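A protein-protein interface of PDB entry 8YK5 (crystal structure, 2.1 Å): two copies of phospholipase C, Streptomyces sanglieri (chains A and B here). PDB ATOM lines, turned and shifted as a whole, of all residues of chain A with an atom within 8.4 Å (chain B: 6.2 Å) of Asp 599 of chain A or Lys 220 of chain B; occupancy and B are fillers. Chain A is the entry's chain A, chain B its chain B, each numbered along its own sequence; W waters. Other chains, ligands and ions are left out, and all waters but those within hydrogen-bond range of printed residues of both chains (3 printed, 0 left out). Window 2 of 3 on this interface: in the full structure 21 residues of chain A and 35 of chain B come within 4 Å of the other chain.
The side-chain amino group (NZ) of Lys 220 of chain B is in salt-bridge range of the side-chain carboxylate (OD2) of Asp 599 of chain A, 3.1 Å away. NE2 of His 628 of chain A lies within hydrogen-bond range of O of Thr 221 of chain B (2.7 Å). A ring nitrogen (ND1) of His 662 of chain A sits at hydrogen-bond distance from the backbone NH of Gly 223 of chain B, 3.4 Å away.
The backbone carbonyl oxygen (O) of Leu 218 of chain B sits at hydrogen-bond distance from the side-chain hydroxyl (OG1) of Thr 221 of chain B (2.6 Å). The side-chain amino group of Lys 220 of chain B is in salt-bridge range of the side-chain carboxylate of Glu 251 of chain B (3.6 Å).
Among the printed residues, pairs that only touch across the chains: His 662 of chain A with Gly 222 of chain B (3.3 Å), His 628 of chain A with Gly 222 of chain B (3.3 Å) and Asp 626 of chain A with Leu 248 of chain B (3.998 Å).
Asp 599 of chain A touches just one residue of chain B: Lys 220. Thr 221 of chain B touches one residue of chain A. Printed residues of chain B within 4 Å of His 628 of chain A: Thr 221 and Gly 222. Printed residues of chain B within 4 Å of Asp 626 of chain A: Leu 248 (3.998 Å). Of the printed residues of chain B, His 662 of chain A touches Gly 222 (3.3 Å) and Gly 223 (3.4 Å). The nearest residue of chain B that does not touch Asp 599 of chain A is Ala 219 of chain B (4.6 Å). The nearest printed residue of chain A that does not touch Leu 248 of chain B is His 628 of chain A (4.6 Å).
Hydrophobic or aromatic side chains of chain B that line the printed part of chain A: Leu 248. Printed residues of chain A that touch a printed residue of chain B: Asp 599, Asp 626, His 628 and His 662. Among the printed residues, 6 pairs touch across the chains. Among the printed residues, Asp or Glu carboxylates within 4 Å of a Lys or Arg side-chain nitrogen of the other chain: Asp 599 of chain A with Lys 220 of chain B (3.1 Å).
No position is printed for both chains. Of the 6 pairs that touch across the chains among the printed residues, none has its exchanged pair printed and touching as well.
Water W3 lies within hydrogen-bond range of O of Asp 626 of chain A (2.6 Å), N of Gly 222 of chain B (3.3 Å) and O of Lys 220 of chain B (3.3 Å). Water W2 bridges the backbone carbonyl oxygen (O) of Ala 627 of chain A and the backbone carbonyl oxygen (O) of Gly 222 of chain B. Water W1 bridges NE2 of His 662 of chain A and O of Ala 219 of chain B.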
ATOM      1  N   PRO A 594      19.487  -2.944  23.338  1.00  0.00           N
ATOM      2  CA  PRO A 594      19.851  -4.205  22.684  1.00  0.00           C
ATOM      3  C   PRO A 594      18.617  -4.887  22.112  1.00  0.00           C
ATOM      4  O   PRO A 594      17.612  -5.058  22.806  1.00  0.00           O
ATOM      5  CB  PRO A 594      20.470  -5.027  23.821  1.00  0.00           C
ATOM      6  CG  PRO A 594      20.762  -4.033  24.911  1.00  0.00           C
ATOM      7  CD  PRO A 594      19.700  -3.005  24.792  1.00  0.00           C
ATOM      8  N   GLY A 596      19.200  -7.985  20.671  1.00  0.00           N
ATOM      9  CA  GLY A 596      19.554  -9.389  20.803  1.00  0.00           C
ATOM     10  C   GLY A 596      20.885  -9.523  21.508  1.00  0.00           C
ATOM     11  O   GLY A 596      21.601  -8.539  21.717  1.00  0.00           O
ATOM     12  N   TYR A 597      21.208 -10.768  21.868  1.00  0.00           N
ATOM     13  CA  TYR A 597      22.447 -11.164  22.538  1.00  0.00           C
ATOM     14  C   TYR A 597      22.528 -10.652  23.970  1.00  0.00           C
ATOM     15  O   TYR A 597      23.604 -10.689  24.575  1.00  0.00           O
ATOM     16  CB  TYR A 597      23.689 -10.724  21.747  1.00  0.00           C
ATOM     17  CG  TYR A 597      23.626 -11.166  20.306  1.00  0.00           C
ATOM     18  CD1 TYR A 597      23.699 -12.508  19.988  1.00  0.00           C
ATOM     19  CD2 TYR A 597      23.448 -10.252  19.274  1.00  0.00           C
ATOM     20  CE1 TYR A 597      23.618 -12.936  18.686  1.00  0.00           C
ATOM     21  CE2 TYR A 597      23.364 -10.668  17.956  1.00  0.00           C
ATOM     22  CZ  TYR A 597      23.449 -12.020  17.672  1.00  0.00           C
ATOM     23  OH  TYR A 597      23.370 -12.489  16.390  1.00  0.00           O
ATOM     24  N   VAL A 598      21.419 -10.180  24.534  1.00  0.00           N
ATOM     25  CA  VAL A 598      21.350  -9.775  25.932  1.00  0.00           C
ATOM     26  C   VAL A 598      20.162 -10.492  26.556  1.00  0.00           C
ATOM     27  O   VAL A 598      19.038 -10.385  26.052  1.00  0.00           O
ATOM     28  CB  VAL A 598      21.218  -8.250  26.082  1.00  0.00           C
ATOM     29  CG1 VAL A 598      21.105  -7.861  27.540  1.00  0.00           C
ATOM     30  CG2 VAL A 598      22.411  -7.561  25.459  1.00  0.00           C
ATOM     31  N   ASP A 599      20.414 -11.248  27.626  1.00  0.00           N
ATOM     32  CA  ASP A 599      19.334 -11.960  28.301  1.00  0.00           C
ATOM     33  C   ASP A 599      18.248 -10.981  28.721  1.00  0.00           C
ATOM     34  O   ASP A 599      18.531  -9.876  29.188  1.00  0.00           O
ATOM     35  CB  ASP A 599      19.869 -12.720  29.516  1.00  0.00           C
ATOM     36  CG  ASP A 599      20.283 -14.144  29.173  1.00  0.00           C
ATOM     37  OD1 ASP A 599      20.214 -14.503  27.970  1.00  0.00           O
ATOM     38  OD2 ASP A 599      20.679 -14.899  30.091  1.00  0.00           O
ATOM     39  N   GLU A 600      16.993 -11.382  28.517  1.00  0.00           N
ATOM     40  CA  GLU A 600      15.894 -10.440  28.685  1.00  0.00           C
ATOM     41  C   GLU A 600      15.838  -9.915  30.112  1.00  0.00           C
ATOM     42  O   GLU A 600      15.613  -8.719  30.329  1.00  0.00           O
ATOM     43  CB  GLU A 600      14.575 -11.098  28.269  1.00  0.00           C
ATOM     44  CG  GLU A 600      13.511 -10.109  27.811  1.00  0.00           C
ATOM     45  CD  GLU A 600      12.511  -9.807  28.906  1.00  0.00           C
ATOM     46  OE1 GLU A 600      12.443 -10.596  29.874  1.00  0.00           O
ATOM     47  OE2 GLU A 600      11.797  -8.784  28.801  1.00  0.00           O
ATOM     48  N   ALA A 601      16.107 -10.765  31.086  1.00  0.00           N
ATOM     49  CA  ALA A 601      16.186 -10.331  32.477  1.00  0.00           C
ATOM     50  C   ALA A 601      17.417  -9.484  32.760  1.00  0.00           C
ATOM     51  O   ALA A 601      18.035  -9.634  33.813  1.00  0.00           O
ATOM     52  CB  ALA A 601      16.139 -11.553  33.395  1.00  0.00           C
ATOM     53  N   ASP A 602      17.786  -8.574  31.857  1.00  0.00           N
ATOM     54  CA  ASP A 602      19.124  -7.987  31.916  1.00  0.00           C
ATOM     55  C   ASP A 602      19.252  -6.789  30.966  1.00  0.00           C
ATOM     56  O   ASP A 602      20.219  -6.020  31.043  1.00  0.00           O
ATOM     57  CB  ASP A 602      20.134  -9.089  31.589  1.00  0.00           C
ATOM     58  CG  ASP A 602      21.543  -8.755  31.988  1.00  0.00           C
ATOM     59  OD1 ASP A 602      22.083  -7.748  31.479  1.00  0.00           O
ATOM     60  OD2 ASP A 602      22.122  -9.526  32.791  1.00  0.00           O
ATOM     61  N   LEU A 603      18.269  -6.611  30.081  1.00  0.00           N
ATOM     62  CA  LEU A 603      18.374  -5.554  29.084  1.00  0.00           C
ATOM     63  C   LEU A 603      18.450  -4.180  29.719  1.00  0.00           C
ATOM     64  O   LEU A 603      19.139  -3.300  29.190  1.00  0.00           O
ATOM     65  CB  LEU A 603      17.191  -5.589  28.112  1.00  0.00           C
ATOM     66  CG  LEU A 603      16.930  -6.896  27.384  1.00  0.00           C
ATOM     67  CD1 LEU A 603      15.451  -7.019  27.074  1.00  0.00           C
ATOM     68  CD2 LEU A 603      17.768  -6.974  26.124  1.00  0.00           C
ATOM     69  N   ARG A 604      17.758  -3.963  30.840  1.00  0.00           N
ATOM     70  CA  ARG A 604      17.713  -2.610  31.386  1.00  0.00           C
ATOM     71  C   ARG A 604      19.090  -2.141  31.836  1.00  0.00           C
ATOM     72  O   ARG A 604      19.430  -0.963  31.661  1.00  0.00           O
ATOM     73  CB  ARG A 604      16.702  -2.558  32.548  1.00  0.00           C
ATOM     74  CG  ARG A 604      16.491  -1.155  33.106  1.00  0.00           C
ATOM     75  CD  ARG A 604      15.182  -1.009  33.884  1.00  0.00           C
ATOM     76  NE  ARG A 604      14.129  -0.359  33.096  1.00  0.00           N
ATOM     77  CZ  ARG A 604      13.315   0.589  33.560  1.00  0.00           C
ATOM     78  NH1 ARG A 604      13.439   1.018  34.812  1.00  0.00           N
ATOM     79  NH2 ARG A 604      12.383   1.118  32.773  1.00  0.00           N
ATOM     80  N   ASP A 605      19.922  -3.055  32.338  1.00  0.00           N
ATOM     81  CA  ASP A 605      21.294  -2.705  32.668  1.00  0.00           C
ATOM     82  C   ASP A 605      22.130  -2.398  31.431  1.00  0.00           C
ATOM     83  O   ASP A 605      23.180  -1.750  31.546  1.00  0.00           O
ATOM     84  CB  ASP A 605      21.933  -3.836  33.468  1.00  0.00           C
ATOM     85  CG  ASP A 605      21.028  -4.361  34.569  1.00  0.00           C
ATOM     86  OD1 ASP A 605      19.897  -4.818  34.254  1.00  0.00           O
ATOM     87  OD2 ASP A 605      21.427  -4.307  35.746  1.00  0.00           O
ATOM     88  N   TRP A 606      21.703  -2.859  30.258  1.00  0.00           N
ATOM     89  CA  TRP A 606      22.430  -2.632  29.024  1.00  0.00           C
ATOM     90  C   TRP A 606      21.727  -1.658  28.096  1.00  0.00           C
ATOM     91  O   TRP A 606      22.306  -1.274  27.075  1.00  0.00           O
ATOM     92  CB  TRP A 606      22.660  -3.964  28.297  1.00  0.00           C
ATOM     93  CG  TRP A 606      23.710  -4.765  28.971  1.00  0.00           C
ATOM     94  CD1 TRP A 606      23.601  -5.423  30.162  1.00  0.00           C
ATOM     95  CD2 TRP A 606      25.054  -4.956  28.528  1.00  0.00           C
ATOM     96  NE1 TRP A 606      24.792  -6.029  30.479  1.00  0.00           N
ATOM     97  CE2 TRP A 606      25.702  -5.758  29.491  1.00  0.00           C
ATOM     98  CE3 TRP A 606      25.772  -4.533  27.408  1.00  0.00           C
ATOM     99  CZ2 TRP A 606      27.034  -6.150  29.366  1.00  0.00           C
ATOM    100  CZ3 TRP A 606      27.093  -4.927  27.281  1.00  0.00           C
ATOM    101  CH2 TRP A 606      27.712  -5.727  28.255  1.00  0.00           C
ATOM    102  N   ASP A 626      30.844 -10.393  26.094  1.00  0.00           N
ATOM    103  CA  ASP A 626      30.051 -11.451  26.718  1.00  0.00           C
ATOM    104  C   ASP A 626      29.333 -12.302  25.682  1.00  0.00           C
ATOM    105  O   ASP A 626      29.068 -13.490  25.926  1.00  0.00           O
ATOM    106  CB  ASP A 626      29.025 -10.855  27.687  1.00  0.00           C
ATOM    107  CG  ASP A 626      29.652 -10.364  28.979  1.00  0.00           C
ATOM    108  OD1 ASP A 626      30.817 -10.729  29.235  1.00  0.00           O
ATOM    109  OD2 ASP A 626      28.980  -9.637  29.745  1.00  0.00           O
ATOM    110  N   ALA A 627      28.999 -11.713  24.531  1.00  0.00           N
ATOM    111  CA  ALA A 627      28.338 -12.408  23.439  1.00  0.00           C
ATOM    112  C   ALA A 627      29.328 -12.863  22.369  1.00  0.00           C
ATOM    113  O   ALA A 627      28.920 -13.187  21.246  1.00  0.00           O
ATOM    114  CB  ALA A 627      27.251 -11.513  22.830  1.00  0.00           C
ATOM    115  N   HIS A 628      30.621 -12.880  22.699  1.00  0.00           N
ATOM    116  CA  HIS A 628      31.672 -13.329  21.788  1.00  0.00           C
ATOM    117  C   HIS A 628      31.683 -12.519  20.497  1.00  0.00           C
ATOM    118  O   HIS A 628      31.876 -13.063  19.409  1.00  0.00           O
ATOM    119  CB  HIS A 628      31.537 -14.826  21.495  1.00  0.00           C
ATOM    120  CG  HIS A 628      31.254 -15.636  22.717  1.00  0.00           C
ATOM    121  ND1 HIS A 628      32.007 -15.523  23.867  1.00  0.00           N
ATOM    122  CD2 HIS A 628      30.275 -16.527  22.995  1.00  0.00           C
ATOM    123  CE1 HIS A 628      31.519 -16.330  24.792  1.00  0.00           C
ATOM    124  NE2 HIS A 628      30.471 -16.956  24.287  1.00  0.00           N
ATOM    125  N   HIS A 662      22.782 -17.399  18.693  1.00  0.00           N
ATOM    126  CA  HIS A 662      22.326 -17.190  20.065  1.00  0.00           C
ATOM    127  C   HIS A 662      21.728 -15.799  20.266  1.00  0.00           C
ATOM    128  O   HIS A 662      21.872 -15.202  21.344  1.00  0.00           O
ATOM    129  CB  HIS A 662      23.466 -17.440  21.053  1.00  0.00           C
ATOM    130  CG  HIS A 662      23.001 -17.777  22.438  1.00  0.00           C
ATOM    131  ND1 HIS A 662      23.349 -17.026  23.546  1.00  0.00           N
ATOM    132  CD2 HIS A 662      22.223 -18.788  22.899  1.00  0.00           C
ATOM    133  CE1 HIS A 662      22.800 -17.558  24.625  1.00  0.00           C
ATOM    134  NE2 HIS A 662      22.113 -18.628  24.261  1.00  0.00           N
ATOM    135  N   HIS A 663      21.103 -15.255  19.219  1.00  0.00           N
ATOM    136  CA  HIS A 663      20.338 -14.014  19.314  1.00  0.00           C
ATOM    137  C   HIS A 663      19.273 -14.090  20.400  1.00  0.00           C
ATOM    138  O   HIS A 663      19.075 -13.135  21.159  1.00  0.00           O
ATOM    139  CB  HIS A 663      19.686 -13.746  17.963  1.00  0.00           C
ATOM    140  CG  HIS A 663      19.358 -12.313  17.712  1.00  0.00           C
ATOM    141  ND1 HIS A 663      20.114 -11.516  16.878  1.00  0.00           N
ATOM    142  CD2 HIS A 663      18.319 -11.547  18.126  1.00  0.00           C
ATOM    143  CE1 HIS A 663      19.568 -10.315  16.805  1.00  0.00           C
ATOM    144  NE2 HIS A 663      18.477 -10.306  17.553  1.00  0.00           N
ATOM    145  N   HIS A 664      18.549 -15.206  20.448  1.00  0.00           N
ATOM    146  CA  HIS A 664      17.540 -15.486  21.460  1.00  0.00           C
ATOM    147  C   HIS A 664      17.576 -16.978  21.795  1.00  0.00           C
ATOM    148  O   HIS A 664      17.276 -17.386  22.916  1.00  0.00           O
ATOM    149  CB  HIS A 664      16.145 -15.088  20.968  1.00  0.00           C
ATOM    150  CG  HIS A 664      15.923 -13.610  20.906  1.00  0.00           C
ATOM    151  ND1 HIS A 664      15.965 -12.899  19.724  1.00  0.00           N
ATOM    152  CD2 HIS A 664      15.658 -12.706  21.879  1.00  0.00           C
ATOM    153  CE1 HIS A 664      15.728 -11.624  19.971  1.00  0.00           C
ATOM    154  NE2 HIS A 664      15.541 -11.479  21.271  1.00  0.00           N
ATOM    155  N   ARG B 215      23.995 -28.055  30.155  1.00  0.00           N
ATOM    156  CA  ARG B 215      23.261 -26.998  29.466  1.00  0.00           C
ATOM    157  C   ARG B 215      22.835 -25.909  30.444  1.00  0.00           C
ATOM    158  O   ARG B 215      22.980 -24.710  30.162  1.00  0.00           O
ATOM    159  CB  ARG B 215      22.046 -27.594  28.752  1.00  0.00           C
ATOM    160  CG  ARG B 215      21.242 -26.599  27.964  1.00  0.00           C
ATOM    161  CD  ARG B 215      20.100 -27.273  27.217  1.00  0.00           C
ATOM    162  NE  ARG B 215      20.565 -28.034  26.062  1.00  0.00           N
ATOM    163  CZ  ARG B 215      20.507 -27.600  24.804  1.00  0.00           C
ATOM    164  NH1 ARG B 215      20.001 -26.402  24.527  1.00  0.00           N
ATOM    165  NH2 ARG B 215      20.956 -28.372  23.822  1.00  0.00           N
ATOM    166  N   LYS B 216      22.331 -26.315  31.609  1.00  0.00           N
ATOM    167  CA  LYS B 216      21.930 -25.360  32.634  1.00  0.00           C
ATOM    168  C   LYS B 216      23.122 -24.566  33.157  1.00  0.00           C
ATOM    169  O   LYS B 216      23.035 -23.345  33.321  1.00  0.00           O
ATOM    170  CB  LYS B 216      21.232 -26.093  33.782  1.00  0.00           C
ATOM    171  CG  LYS B 216      20.594 -25.169  34.791  1.00  0.00           C
ATOM    172  CD  LYS B 216      19.796 -25.945  35.827  1.00  0.00           C
ATOM    173  CE  LYS B 216      19.103 -24.983  36.797  1.00  0.00           C
ATOM    174  NZ  LYS B 216      18.467 -25.702  37.927  1.00  0.00           N
ATOM    175  N   ALA B 217      24.246 -25.239  33.429  1.00  0.00           N
ATOM    176  CA  ALA B 217      25.406 -24.531  33.972  1.00  0.00           C
ATOM    177  C   ALA B 217      26.046 -23.591  32.955  1.00  0.00           C
ATOM    178  O   ALA B 217      26.744 -22.654  33.357  1.00  0.00           O
ATOM    179  CB  ALA B 217      26.448 -25.524  34.484  1.00  0.00           C
ATOM    180  N   LEU B 218      25.818 -23.818  31.656  1.00  0.00           N
ATOM    181  CA  LEU B 218      26.381 -23.008  30.582  1.00  0.00           C
ATOM    182  C   LEU B 218      25.413 -21.953  30.064  1.00  0.00           C
ATOM    183  O   LEU B 218      25.715 -21.292  29.066  1.00  0.00           O
ATOM    184  CB  LEU B 218      26.814 -23.896  29.418  1.00  0.00           C
ATOM    185  CG  LEU B 218      27.916 -24.919  29.667  1.00  0.00           C
ATOM    186  CD1 LEU B 218      27.996 -25.875  28.496  1.00  0.00           C
ATOM    187  CD2 LEU B 218      29.248 -24.205  29.894  1.00  0.00           C
ATOM    188  N   ALA B 219      24.261 -21.781  30.720  1.00  0.00           N
ATOM    189  CA  ALA B 219      23.176 -20.976  30.170  1.00  0.00           C
ATOM    190  C   ALA B 219      23.538 -19.498  30.002  1.00  0.00           C
ATOM    191  O   ALA B 219      22.920 -18.810  29.181  1.00  0.00           O
ATOM    192  CB  ALA B 219      21.947 -21.120  31.073  1.00  0.00           C
ATOM    193  N   LYS B 220      24.512 -18.986  30.753  1.00  0.00           N
ATOM    194  CA  LYS B 220      24.918 -17.598  30.623  1.00  0.00           C
ATOM    195  C   LYS B 220      26.189 -17.421  29.799  1.00  0.00           C
ATOM    196  O   LYS B 220      26.728 -16.313  29.759  1.00  0.00           O
ATOM    197  CB  LYS B 220      25.093 -16.964  32.007  1.00  0.00           C
ATOM    198  CG  LYS B 220      23.782 -16.743  32.759  1.00  0.00           C
ATOM    199  CD  LYS B 220      23.001 -15.601  32.136  1.00  0.00           C
ATOM    200  CE  LYS B 220      21.987 -14.978  33.092  1.00  0.00           C
ATOM    201  NZ  LYS B 220      21.682 -13.568  32.693  1.00  0.00           N
ATOM    202  N   THR B 221      26.671 -18.468  29.124  1.00  0.00           N
ATOM    203  CA  THR B 221      27.951 -18.365  28.426  1.00  0.00           C
ATOM    204  C   THR B 221      27.832 -17.839  26.999  1.00  0.00           C
ATOM    205  O   THR B 221      28.841 -17.775  26.289  1.00  0.00           O
ATOM    206  CB  THR B 221      28.677 -19.722  28.427  1.00  0.00           C
ATOM    207  OG1 THR B 221      27.908 -20.702  27.718  1.00  0.00           O
ATOM    208  CG2 THR B 221      28.923 -20.205  29.870  1.00  0.00           C
ATOM    209  N   GLY B 222      26.645 -17.440  26.561  1.00  0.00           N
ATOM    210  CA  GLY B 222      26.538 -16.785  25.273  1.00  0.00           C
ATOM    211  C   GLY B 222      26.557 -17.707  24.073  1.00  0.00           C
ATOM    212  O   GLY B 222      27.038 -17.307  23.005  1.00  0.00           O
ATOM    213  N   GLY B 223      26.053 -18.933  24.212  1.00  0.00           N
ATOM    214  CA  GLY B 223      25.923 -19.816  23.065  1.00  0.00           C
ATOM    215  C   GLY B 223      26.326 -21.262  23.287  1.00  0.00           C
ATOM    216  O   GLY B 223      25.954 -22.128  22.496  1.00  0.00           O
ATOM    217  N   LEU B 248      31.238 -16.057  33.319  1.00  0.00           N
ATOM    218  CA  LEU B 248      30.003 -16.481  32.671  1.00  0.00           C
ATOM    219  C   LEU B 248      29.592 -17.887  33.108  1.00  0.00           C
ATOM    220  O   LEU B 248      28.410 -18.138  33.373  1.00  0.00           O
ATOM    221  CB  LEU B 248      30.174 -16.405  31.150  1.00  0.00           C
ATOM    222  CG  LEU B 248      30.397 -14.994  30.587  1.00  0.00           C
ATOM    223  CD1 LEU B 248      30.896 -14.999  29.146  1.00  0.00           C
ATOM    224  CD2 LEU B 248      29.123 -14.191  30.695  1.00  0.00           C
ATOM    225  N   LEU B 249      30.551 -18.818  33.201  1.00  0.00           N
ATOM    226  CA  LEU B 249      30.225 -20.167  33.671  1.00  0.00           C
ATOM    227  C   LEU B 249      29.672 -20.142  35.095  1.00  0.00           C
ATOM    228  O   LEU B 249      28.648 -20.777  35.386  1.00  0.00           O
ATOM    229  CB  LEU B 249      31.456 -21.080  33.601  1.00  0.00           C
ATOM    230  CG  LEU B 249      31.296 -22.437  34.323  1.00  0.00           C
ATOM    231  CD1 LEU B 249      30.159 -23.257  33.708  1.00  0.00           C
ATOM    232  CD2 LEU B 249      32.591 -23.261  34.349  1.00  0.00           C
ATOM    233  N   GLU B 251      28.114 -17.983  36.752  1.00  0.00           N
ATOM    234  CA  GLU B 251      26.751 -17.470  36.837  1.00  0.00           C
ATOM    235  C   GLU B 251      25.731 -18.583  36.615  1.00  0.00           C
ATOM    236  O   GLU B 251      24.721 -18.664  37.325  1.00  0.00           O
ATOM    237  CB  GLU B 251      26.559 -16.344  35.816  1.00  0.00           C
ATOM    238  CG  GLU B 251      25.694 -15.197  36.297  1.00  0.00           C
ATOM    239  CD  GLU B 251      25.448 -14.165  35.219  1.00  0.00           C
ATOM    240  OE1 GLU B 251      26.378 -13.897  34.413  1.00  0.00           O
ATOM    241  OE2 GLU B 251      24.315 -13.632  35.176  1.00  0.00           O
ATOM    242  N   GLY B 252      25.978 -19.456  35.641  1.00  0.00           N
ATOM    243  CA  GLY B 252      25.079 -20.578  35.442  1.00  0.00           C
ATOM    244  C   GLY B 252      25.229 -21.630  36.522  1.00  0.00           C
ATOM    245  O   GLY B 252      24.244 -22.236  36.956  1.00  0.00           O
HETATM  246  O   HOH W   1      22.159 -20.308  26.644  1.00  0.00           O
HETATM  247  O   HOH W   2      26.721 -14.995  21.254  1.00  0.00           O
HETATM  248  O   HOH W   3      26.891 -14.191  27.188  1.00  0.00           O
